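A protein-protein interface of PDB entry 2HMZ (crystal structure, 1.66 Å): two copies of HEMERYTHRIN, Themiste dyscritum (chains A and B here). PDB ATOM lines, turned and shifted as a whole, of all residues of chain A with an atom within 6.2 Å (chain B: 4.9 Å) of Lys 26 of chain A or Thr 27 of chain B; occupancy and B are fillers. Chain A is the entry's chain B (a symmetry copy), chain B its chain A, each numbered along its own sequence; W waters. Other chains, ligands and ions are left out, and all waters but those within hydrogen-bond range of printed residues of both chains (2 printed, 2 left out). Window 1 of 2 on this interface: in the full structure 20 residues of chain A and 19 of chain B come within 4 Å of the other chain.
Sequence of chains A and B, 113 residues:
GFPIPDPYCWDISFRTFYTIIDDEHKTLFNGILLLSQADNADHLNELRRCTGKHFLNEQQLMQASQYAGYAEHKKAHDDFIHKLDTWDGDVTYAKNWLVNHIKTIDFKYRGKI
NZ of Lys 26 of chain B lies within salt-bridge range of OD2 of Asp 23 of chain B (2.8 Å).
OG1 of Thr 27 of chain B lies within hydrogen-bond range of O of Glu 24 of chain B (2.6 Å).
The guanidinium group (NH1) of Arg 49 of chain B lies within salt-bridge range of the side-chain carboxylate (OE1) of Glu 46 of chain B, at 2.9 Å.
The backbone carbonyl oxygen (O) of Glu 46 of chain B lies within hydrogen-bond range of the side-chain sulfur (SG) of Cys 50 of chain B (3.3 Å).
The side-chain carboxylate (OD2) of Asp 23 of chain A is in salt-bridge range of the side-chain amino group (NZ) of Lys 26 of chain A, 3.0 Å away.
The backbone carbonyl oxygen (O) of Glu 24 of chain A lies within hydrogen-bond range of the side-chain hydroxyl (OG1) of Thr 27 of chain A, 2.6 Å away.
Asp 23 of chain A touches Thr 27 of chain B, and with the chains exchanged Thr 27 of chain A touches Asp 23 of chain B.
Lys 26 of chain A touches Thr 27 of chain B, but with the chains exchanged Thr 27 of chain A does not touch Lys 26 of chain B (4.01 Å).
Lys 26 of chain A touches Asn 30 of chain B, and with the chains exchanged Asn 30 of chain A touches Lys 26 of chain B.
Of the 14 pairs that touch across the chains among the printed residues, 4 have their exchanged pair printed and touching as well.
The backbone carbonyl oxygen (O) of Trp 10 of chain A lies close to the side-chain amide oxygen (OD1) of Asn 30 of chain B (3.0 Å).
The side-chain amino group (NZ) of Lys 26 of chain A is in salt-bridge range of the side-chain carboxylate (OE1) of Glu 46 of chain B, 2.6 Å away.
The guanidinium group (NH1) of Arg 49 of chain B is in salt-bridge range of the side-chain carboxylate (OD2) of Asp 23 of chain A, at 2.9 Å.
The side-chain sulfur (SG) of Cys 50 of chain B is in hydrogen-bond range of the side-chain carboxylate (OD2) of Asp 23 of chain A, 3.4 Å away.
The side-chain amino group (NZ) of Lys 26 of chain A lies within hydrogen-bond range of the side-chain sulfur (SG) of Cys 50 of chain B.
The side-chain amino group (NZ) of Lys 53 of chain B is in salt-bridge range of the side-chain carboxylate (OD1) of Asp 23 of chain A, 2.7 Å away.
Glu 46 of chain B touches Trp 10 of chain A (OE1 to CH2, 3.8 Å).
Thr 19 of chain A touches Arg 49 of chain B.
Asp 23 of chain A touches Thr 27 of chain B.
CG2 of Thr 27 of chain B touches CD of Lys 26 of chain A (3.98 Å).
Lys 26 of chain A touches Asn 30 of chain B (CD to ND2, 3.8 Å).
NH1 of Arg 49 of chain B touches NZ of Lys 26 of chain A, at 3.6 Å.
Asp 23 of chain B touches Thr 27 of chain A (O to CG2, 3.9 Å).
CD of Lys 26 of chain B touches ND2 of Asn 30 of chain A, at 3.7 Å.
Water W1 lies within hydrogen-bond range of OD2 of Asp 22 of chain A and OE1 of Glu 46 of chain B.
Water W2 bridges OD1 of Asp 23 of chain A (2.8 Å) and NZ of Lys 53 of chain B (3.0 Å).
Printed residues of chain B within 4 Å of Thr 19 of chain A: Arg 49.
Ile 21 of chain A touches none of the printed residues of chain B.
Lys 26 of chain A touches just these residues of chain B: Thr 27 (3.98 Å), Asn 30 (3.8 Å), Glu 46 (2.6 Å), Arg 49 (3.6 Å) and Cys 50 (3.5 Å).
Printed residues of chain A within 4 Å of Lys 26 of chain B: Asn 30 (3.7 Å).
Thr 27 of chain B touches just these residues of chain A: Asp 23 (3.9 Å) and Lys 26 (3.98 Å).
Of the printed residues of chain A, Asn 30 of chain B touches Trp 10 (3.0 Å) and Lys 26 (3.8 Å).
Of the printed residues of chain A, Lys 53 of chain B touches Asp 23 (2.7 Å).
Of the 13 printed residues of chain A, 6 touch a printed residue of chain B.
Hydrophobic or aromatic side chains of chain A within 4 Å of the printed part of chain B: Trp 10.
Printed residues of chain B that touch a printed residue of chain A: Asp 23, Lys 26, Thr 27, Asn 30, Glu 46, Arg 49, Cys 50 and Lys 53.
Among the printed residues, 14 pairs touch across the chains.
Among the printed residues, Asp or Glu carboxylates within 4 Å of a Lys or Arg side-chain nitrogen of the other chain: Asp 23 of chain A with Arg 49 of chain B, Asp 23 of chain A with Lys 53 of chain B and Lys 26 of chain A with Glu 46 of chain B.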
ATOM      1  N   TRP A  10       2.805  24.333  -5.741  1.00  0.00           N
ATOM      2  CA  TRP A  10       3.165  25.744  -5.888  1.00  0.00           C
ATOM      3  C   TRP A  10       2.088  26.625  -5.351  1.00  0.00           C
ATOM      4  O   TRP A  10       0.858  26.307  -5.532  1.00  0.00           O
ATOM      5  CB  TRP A  10       3.430  25.904  -7.395  1.00  0.00           C
ATOM      6  CG  TRP A  10       3.917  27.299  -7.752  1.00  0.00           C
ATOM      7  CD1 TRP A  10       5.228  27.659  -7.958  1.00  0.00           C
ATOM      8  CD2 TRP A  10       3.092  28.382  -8.128  1.00  0.00           C
ATOM      9  NE1 TRP A  10       5.246  28.932  -8.437  1.00  0.00           N
ATOM     10  CE2 TRP A  10       4.000  29.429  -8.522  1.00  0.00           C
ATOM     11  CE3 TRP A  10       1.714  28.597  -8.147  1.00  0.00           C
ATOM     12  CZ2 TRP A  10       3.504  30.681  -8.953  1.00  0.00           C
ATOM     13  CZ3 TRP A  10       1.235  29.835  -8.556  1.00  0.00           C
ATOM     14  CH2 TRP A  10       2.135  30.837  -8.924  1.00  0.00           C
ATOM     15  N   THR A  19       6.188  34.787 -15.976  1.00  0.00           N
ATOM     16  CA  THR A  19       5.216  33.655 -16.143  1.00  0.00           C
ATOM     17  C   THR A  19       5.852  32.420 -16.655  1.00  0.00           C
ATOM     18  O   THR A  19       5.441  31.304 -16.154  1.00  0.00           O
ATOM     19  CB  THR A  19       3.931  34.106 -16.958  1.00  0.00           C
ATOM     20  OG1 THR A  19       4.438  34.299 -18.299  1.00  0.00           O
ATOM     21  CG2 THR A  19       3.210  35.332 -16.442  1.00  0.00           C
ATOM     22  N   ILE A  21       8.842  31.272 -16.042  1.00  0.00           N
ATOM     23  CA  ILE A  21       9.563  30.760 -14.874  1.00  0.00           C
ATOM     24  C   ILE A  21       8.573  30.175 -13.864  1.00  0.00           C
ATOM     25  O   ILE A  21       8.757  29.020 -13.437  1.00  0.00           O
ATOM     26  CB  ILE A  21      10.429  31.889 -14.264  1.00  0.00           C
ATOM     27  CG1 ILE A  21      11.597  32.298 -15.231  1.00  0.00           C
ATOM     28  CG2 ILE A  21      10.999  31.563 -12.892  1.00  0.00           C
ATOM     29  CD1 ILE A  21      12.765  31.391 -15.398  1.00  0.00           C
ATOM     30  N   ASP A  22       7.530  30.918 -13.582  1.00  0.00           N
ATOM     31  CA  ASP A  22       6.565  30.432 -12.599  1.00  0.00           C
ATOM     32  C   ASP A  22       6.022  29.104 -13.095  1.00  0.00           C
ATOM     33  O   ASP A  22       5.730  28.252 -12.263  1.00  0.00           O
ATOM     34  CB  ASP A  22       5.459  31.452 -12.366  1.00  0.00           C
ATOM     35  CG  ASP A  22       6.000  32.728 -11.637  1.00  0.00           C
ATOM     36  OD1 ASP A  22       6.987  32.602 -10.938  1.00  0.00           O
ATOM     37  OD2 ASP A  22       5.222  33.667 -11.649  1.00  0.00           O
ATOM     38  N   ASP A  23       5.656  29.047 -14.383  1.00  0.00           N
ATOM     39  CA  ASP A  23       5.062  27.765 -14.902  1.00  0.00           C
ATOM     40  C   ASP A  23       6.037  26.616 -14.779  1.00  0.00           C
ATOM     41  O   ASP A  23       5.616  25.467 -14.478  1.00  0.00           O
ATOM     42  CB  ASP A  23       4.492  27.952 -16.292  1.00  0.00           C
ATOM     43  CG  ASP A  23       3.219  28.725 -16.363  1.00  0.00           C
ATOM     44  OD1 ASP A  23       2.867  29.204 -17.459  1.00  0.00           O
ATOM     45  OD2 ASP A  23       2.593  28.988 -15.299  1.00  0.00           O
ATOM     46  N   GLU A  24       7.308  26.799 -15.114  1.00  0.00           N
ATOM     47  CA  GLU A  24       8.311  25.781 -14.867  1.00  0.00           C
ATOM     48  C   GLU A  24       8.416  25.403 -13.389  1.00  0.00           C
ATOM     49  O   GLU A  24       8.519  24.211 -13.041  1.00  0.00           O
ATOM     50  CB  GLU A  24       9.692  26.270 -15.325  1.00  0.00           C
ATOM     51  CG  GLU A  24       9.685  26.291 -16.845  1.00  0.00           C
ATOM     52  CD  GLU A  24      10.971  26.780 -17.456  1.00  0.00           C
ATOM     53  OE1 GLU A  24      11.039  26.820 -18.695  1.00  0.00           O
ATOM     54  OE2 GLU A  24      11.889  27.204 -16.728  1.00  0.00           O
ATOM     55  N   HIS A  25       8.378  26.421 -12.518  1.00  0.00           N
ATOM     56  CA  HIS A  25       8.424  26.115 -11.049  1.00  0.00           C
ATOM     57  C   HIS A  25       7.317  25.197 -10.609  1.00  0.00           C
ATOM     58  O   HIS A  25       7.561  24.310  -9.737  1.00  0.00           O
ATOM     59  CB  HIS A  25       8.415  27.424 -10.183  1.00  0.00           C
ATOM     60  CG  HIS A  25       9.741  28.118 -10.248  1.00  0.00           C
ATOM     61  ND1 HIS A  25       9.862  29.443  -9.904  1.00  0.00           N
ATOM     62  CD2 HIS A  25      10.925  27.736 -10.699  1.00  0.00           C
ATOM     63  CE1 HIS A  25      11.145  29.743  -9.981  1.00  0.00           C
ATOM     64  NE2 HIS A  25      11.859  28.746 -10.451  1.00  0.00           N
ATOM     65  N   LYS A  26       6.116  25.337 -11.135  1.00  0.00           N
ATOM     66  CA  LYS A  26       4.963  24.500 -10.789  1.00  0.00           C
ATOM     67  C   LYS A  26       5.330  23.043 -11.098  1.00  0.00           C
ATOM     68  O   LYS A  26       4.925  22.167 -10.339  1.00  0.00           O
ATOM     69  CB  LYS A  26       3.679  24.906 -11.539  1.00  0.00           C
ATOM     70  CG  LYS A  26       3.255  26.329 -11.183  1.00  0.00           C
ATOM     71  CD  LYS A  26       2.217  26.890 -12.143  1.00  0.00           C
ATOM     72  CE  LYS A  26       1.960  28.355 -11.867  1.00  0.00           C
ATOM     73  NZ  LYS A  26       0.960  28.930 -12.790  1.00  0.00           N
ATOM     74  N   THR A  27       6.101  22.820 -12.148  1.00  0.00           N
ATOM     75  CA  THR A  27       6.483  21.448 -12.469  1.00  0.00           C
ATOM     76  C   THR A  27       7.440  20.832 -11.465  1.00  0.00           C
ATOM     77  O   THR A  27       7.472  19.569 -11.326  1.00  0.00           O
ATOM     78  CB  THR A  27       7.007  21.290 -13.947  1.00  0.00           C
ATOM     79  OG1 THR A  27       8.355  21.847 -14.012  1.00  0.00           O
ATOM     80  CG2 THR A  27       6.034  21.919 -14.959  1.00  0.00           C
ATOM     81  N   LEU A  28       8.283  21.623 -10.870  1.00  0.00           N
ATOM     82  CA  LEU A  28       9.278  21.168  -9.880  1.00  0.00           C
ATOM     83  C   LEU A  28       8.491  20.760  -8.604  1.00  0.00           C
ATOM     84  O   LEU A  28       8.782  19.706  -8.048  1.00  0.00           O
ATOM     85  CB  LEU A  28      10.344  22.204  -9.710  1.00  0.00           C
ATOM     86  CG  LEU A  28      11.228  22.722 -10.807  1.00  0.00           C
ATOM     87  CD1 LEU A  28      12.351  23.556 -10.205  1.00  0.00           C
ATOM     88  CD2 LEU A  28      11.791  21.557 -11.593  1.00  0.00           C
ATOM     89  N   PHE A  29       7.576  21.621  -8.186  1.00  0.00           N
ATOM     90  CA  PHE A  29       6.753  21.250  -7.017  1.00  0.00           C
ATOM     91  C   PHE A  29       6.075  19.900  -7.253  1.00  0.00           C
ATOM     92  O   PHE A  29       6.030  19.004  -6.372  1.00  0.00           O
ATOM     93  CB  PHE A  29       5.712  22.312  -6.689  1.00  0.00           C
ATOM     94  CG  PHE A  29       6.255  23.423  -5.869  1.00  0.00           C
ATOM     95  CD1 PHE A  29       6.880  24.511  -6.452  1.00  0.00           C
ATOM     96  CD2 PHE A  29       6.083  23.377  -4.454  1.00  0.00           C
ATOM     97  CE1 PHE A  29       7.379  25.562  -5.680  1.00  0.00           C
ATOM     98  CE2 PHE A  29       6.672  24.350  -3.658  1.00  0.00           C
ATOM     99  CZ  PHE A  29       7.245  25.479  -4.270  1.00  0.00           C
ATOM    100  N   ASN A  30       5.478  19.767  -8.419  1.00  0.00           N
ATOM    101  CA  ASN A  30       4.745  18.512  -8.765  1.00  0.00           C
ATOM    102  C   ASN A  30       5.721  17.325  -8.739  1.00  0.00           C
ATOM    103  O   ASN A  30       5.294  16.278  -8.235  1.00  0.00           O
ATOM    104  CB  ASN A  30       4.100  18.665 -10.118  1.00  0.00           C
ATOM    105  CG  ASN A  30       3.486  17.335 -10.622  1.00  0.00           C
ATOM    106  OD1 ASN A  30       2.425  17.059 -10.023  1.00  0.00           O
ATOM    107  ND2 ASN A  30       4.202  16.616 -11.435  1.00  0.00           N
ATOM    108  N   GLY A  31       6.922  17.497  -9.280  1.00  0.00           N
ATOM    109  CA  GLY A  31       7.898  16.421  -9.343  1.00  0.00           C
ATOM    110  C   GLY A  31       8.224  15.898  -7.917  1.00  0.00           C
ATOM    111  O   GLY A  31       8.243  14.663  -7.746  1.00  0.00           O
ATOM    112  N   ASP B  23       3.773  19.144 -19.200  1.00  0.00           N
ATOM    113  CA  ASP B  23       4.197  20.293 -18.315  1.00  0.00           C
ATOM    114  C   ASP B  23       3.127  21.324 -18.269  1.00  0.00           C
ATOM    115  O   ASP B  23       2.882  21.902 -17.193  1.00  0.00           O
ATOM    116  CB  ASP B  23       5.552  20.792 -18.712  1.00  0.00           C
ATOM    117  CG  ASP B  23       6.669  19.817 -18.431  1.00  0.00           C
ATOM    118  OD1 ASP B  23       7.765  19.964 -18.957  1.00  0.00           O
ATOM    119  OD2 ASP B  23       6.451  18.859 -17.624  1.00  0.00           O
ATOM    120  N   GLU B  24       2.454  21.611 -19.376  1.00  0.00           N
ATOM    121  CA  GLU B  24       1.342  22.571 -19.317  1.00  0.00           C
ATOM    122  C   GLU B  24       0.207  22.015 -18.505  1.00  0.00           C
ATOM    123  O   GLU B  24      -0.396  22.761 -17.708  1.00  0.00           O
ATOM    124  CB  GLU B  24       0.839  22.870 -20.743  1.00  0.00           C
ATOM    125  CG  GLU B  24       1.862  23.680 -21.540  1.00  0.00           C
ATOM    126  CD  GLU B  24       1.469  24.132 -22.907  1.00  0.00           C
ATOM    127  OE1 GLU B  24       2.223  24.920 -23.509  1.00  0.00           O
ATOM    128  OE2 GLU B  24       0.452  23.636 -23.415  1.00  0.00           O
ATOM    129  N   HIS B  25      -0.094  20.732 -18.698  1.00  0.00           N
ATOM    130  CA  HIS B  25      -1.204  20.131 -17.905  1.00  0.00           C
ATOM    131  C   HIS B  25      -0.986  20.232 -16.406  1.00  0.00           C
ATOM    132  O   HIS B  25      -1.988  20.536 -15.690  1.00  0.00           O
ATOM    133  CB  HIS B  25      -1.451  18.654 -18.258  1.00  0.00           C
ATOM    134  CG  HIS B  25      -2.089  18.471 -19.619  1.00  0.00           C
ATOM    135  ND1 HIS B  25      -2.070  17.286 -20.298  1.00  0.00           N
ATOM    136  CD2 HIS B  25      -2.697  19.354 -20.428  1.00  0.00           C
ATOM    137  CE1 HIS B  25      -2.789  17.444 -21.425  1.00  0.00           C
ATOM    138  NE2 HIS B  25      -3.211  18.694 -21.546  1.00  0.00           N
ATOM    139  N   LYS B  26       0.220  20.140 -15.948  1.00  0.00           N
ATOM    140  CA  LYS B  26       0.565  20.292 -14.506  1.00  0.00           C
ATOM    141  C   LYS B  26       0.113  21.639 -14.033  1.00  0.00           C
ATOM    142  O   LYS B  26      -0.364  21.808 -12.932  1.00  0.00           O
ATOM    143  CB  LYS B  26       2.061  20.069 -14.351  1.00  0.00           C
ATOM    144  CG  LYS B  26       2.508  18.623 -14.558  1.00  0.00           C
ATOM    145  CD  LYS B  26       4.010  18.477 -14.589  1.00  0.00           C
ATOM    146  CE  LYS B  26       4.426  17.170 -15.241  1.00  0.00           C
ATOM    147  NZ  LYS B  26       5.876  17.113 -15.457  1.00  0.00           N
ATOM    148  N   THR B  27       0.240  22.690 -14.843  1.00  0.00           N
ATOM    149  CA  THR B  27      -0.143  24.023 -14.456  1.00  0.00           C
ATOM    150  C   THR B  27      -1.636  24.093 -14.302  1.00  0.00           C
ATOM    151  O   THR B  27      -2.101  24.901 -13.463  1.00  0.00           O
ATOM    152  CB  THR B  27       0.445  25.166 -15.406  1.00  0.00           C
ATOM    153  OG1 THR B  27      -0.306  25.148 -16.691  1.00  0.00           O
ATOM    154  CG2 THR B  27       1.928  25.064 -15.665  1.00  0.00           C
ATOM    155  N   LEU B  28      -2.446  23.336 -15.030  1.00  0.00           N
ATOM    156  CA  LEU B  28      -3.908  23.437 -14.958  1.00  0.00           C
ATOM    157  C   LEU B  28      -4.325  22.748 -13.647  1.00  0.00           C
ATOM    158  O   LEU B  28      -5.199  23.316 -12.999  1.00  0.00           O
ATOM    159  CB  LEU B  28      -4.519  22.881 -16.198  1.00  0.00           C
ATOM    160  CG  LEU B  28      -4.017  23.506 -17.529  1.00  0.00           C
ATOM    161  CD1 LEU B  28      -4.958  22.907 -18.612  1.00  0.00           C
ATOM    162  CD2 LEU B  28      -4.115  24.961 -17.567  1.00  0.00           C
ATOM    163  N   PHE B  29      -3.748  21.634 -13.311  1.00  0.00           N
ATOM    164  CA  PHE B  29      -4.080  21.003 -11.992  1.00  0.00           C
ATOM    165  C   PHE B  29      -3.813  22.019 -10.868  1.00  0.00           C
ATOM    166  O   PHE B  29      -4.616  22.221  -9.976  1.00  0.00           O
ATOM    167  CB  PHE B  29      -3.235  19.758 -11.768  1.00  0.00           C
ATOM    168  CG  PHE B  29      -3.838  18.589 -12.500  1.00  0.00           C
ATOM    169  CD1 PHE B  29      -3.561  18.359 -13.829  1.00  0.00           C
ATOM    170  CD2 PHE B  29      -4.735  17.773 -11.755  1.00  0.00           C
ATOM    171  CE1 PHE B  29      -4.052  17.216 -14.458  1.00  0.00           C
ATOM    172  CE2 PHE B  29      -5.322  16.679 -12.398  1.00  0.00           C
ATOM    173  CZ  PHE B  29      -4.974  16.454 -13.758  1.00  0.00           C
ATOM    174  N   ASN B  30      -2.608  22.579 -10.913  1.00  0.00           N
ATOM    175  CA  ASN B  30      -2.228  23.588  -9.913  1.00  0.00           C
ATOM    176  C   ASN B  30      -3.217  24.754  -9.859  1.00  0.00           C
ATOM    177  O   ASN B  30      -3.580  25.147  -8.714  1.00  0.00           O
ATOM    178  CB  ASN B  30      -0.799  24.114 -10.151  1.00  0.00           C
ATOM    179  CG  ASN B  30      -0.388  25.183  -9.092  1.00  0.00           C
ATOM    180  OD1 ASN B  30      -0.057  24.767  -7.968  1.00  0.00           O
ATOM    181  ND2 ASN B  30      -0.529  26.422  -9.490  1.00  0.00           N
ATOM    182  N   GLY B  31      -3.659  25.369 -10.944  1.00  0.00           N
ATOM    183  CA  GLY B  31      -4.593  26.486 -10.922  1.00  0.00           C
ATOM    184  C   GLY B  31      -5.928  26.080 -10.232  1.00  0.00           C
ATOM    185  O   GLY B  31      -6.476  26.885  -9.486  1.00  0.00           O
ATOM    186  N   GLU B  46      -4.500  33.177 -12.510  1.00  0.00           N
ATOM    187  CA  GLU B  46      -3.453  32.181 -12.760  1.00  0.00           C
ATOM    188  C   GLU B  46      -3.951  31.014 -13.611  1.00  0.00           C
ATOM    189  O   GLU B  46      -3.409  30.565 -14.649  1.00  0.00           O
ATOM    190  CB  GLU B  46      -2.918  31.694 -11.407  1.00  0.00           C
ATOM    191  CG  GLU B  46      -1.521  31.118 -11.458  1.00  0.00           C
ATOM    192  CD  GLU B  46      -0.369  31.915 -11.909  1.00  0.00           C
ATOM    193  OE1 GLU B  46       0.656  31.494 -12.394  1.00  0.00           O
ATOM    194  OE2 GLU B  46      -0.486  33.163 -11.689  1.00  0.00           O
ATOM    195  N   ARG B  49      -4.939  32.288 -17.170  1.00  0.00           N
ATOM    196  CA  ARG B  49      -3.780  32.530 -18.054  1.00  0.00           C
ATOM    197  C   ARG B  49      -3.266  31.163 -18.536  1.00  0.00           C
ATOM    198  O   ARG B  49      -3.056  30.971 -19.748  1.00  0.00           O
ATOM    199  CB  ARG B  49      -2.676  33.302 -17.372  1.00  0.00           C
ATOM    200  CG  ARG B  49      -1.404  33.464 -18.194  1.00  0.00           C
ATOM    201  CD  ARG B  49      -0.303  34.093 -17.374  1.00  0.00           C
ATOM    202  NE  ARG B  49       0.209  33.347 -16.236  1.00  0.00           N
ATOM    203  CZ  ARG B  49       0.934  32.222 -16.305  1.00  0.00           C
ATOM    204  NH1 ARG B  49       1.418  31.609 -15.200  1.00  0.00           N
ATOM    205  NH2 ARG B  49       1.341  31.723 -17.511  1.00  0.00           N
ATOM    206  N   CYS B  50      -3.015  30.264 -17.621  1.00  0.00           N
ATOM    207  CA  CYS B  50      -2.451  28.955 -17.976  1.00  0.00           C
ATOM    208  C   CYS B  50      -3.355  28.162 -18.893  1.00  0.00           C
ATOM    209  O   CYS B  50      -2.878  27.447 -19.813  1.00  0.00           O
ATOM    210  CB  CYS B  50      -2.160  28.168 -16.682  1.00  0.00           C
ATOM    211  SG  CYS B  50      -0.806  28.862 -15.804  1.00  0.00           S
ATOM    212  N   LYS B  53      -3.348  29.800 -22.524  1.00  0.00           N
ATOM    213  CA  LYS B  53      -2.052  29.515 -23.163  1.00  0.00           C
ATOM    214  C   LYS B  53      -2.011  28.023 -23.538  1.00  0.00           C
ATOM    215  O   LYS B  53      -1.612  27.660 -24.692  1.00  0.00           O
ATOM    216  CB  LYS B  53      -0.919  29.851 -22.225  1.00  0.00           C
ATOM    217  CG  LYS B  53       0.478  29.492 -22.672  1.00  0.00           C
ATOM    218  CD  LYS B  53       1.438  29.585 -21.438  1.00  0.00           C
ATOM    219  CE  LYS B  53       2.131  28.336 -21.076  1.00  0.00           C
ATOM    220  NZ  LYS B  53       2.101  27.863 -19.667  1.00  0.00           N
HETATM  221  O   HOH W   1       2.493  33.793 -11.875  1.00  0.00           O
HETATM  222  O   HOH W   2       4.420  29.797 -19.661  1.00  0.00           O
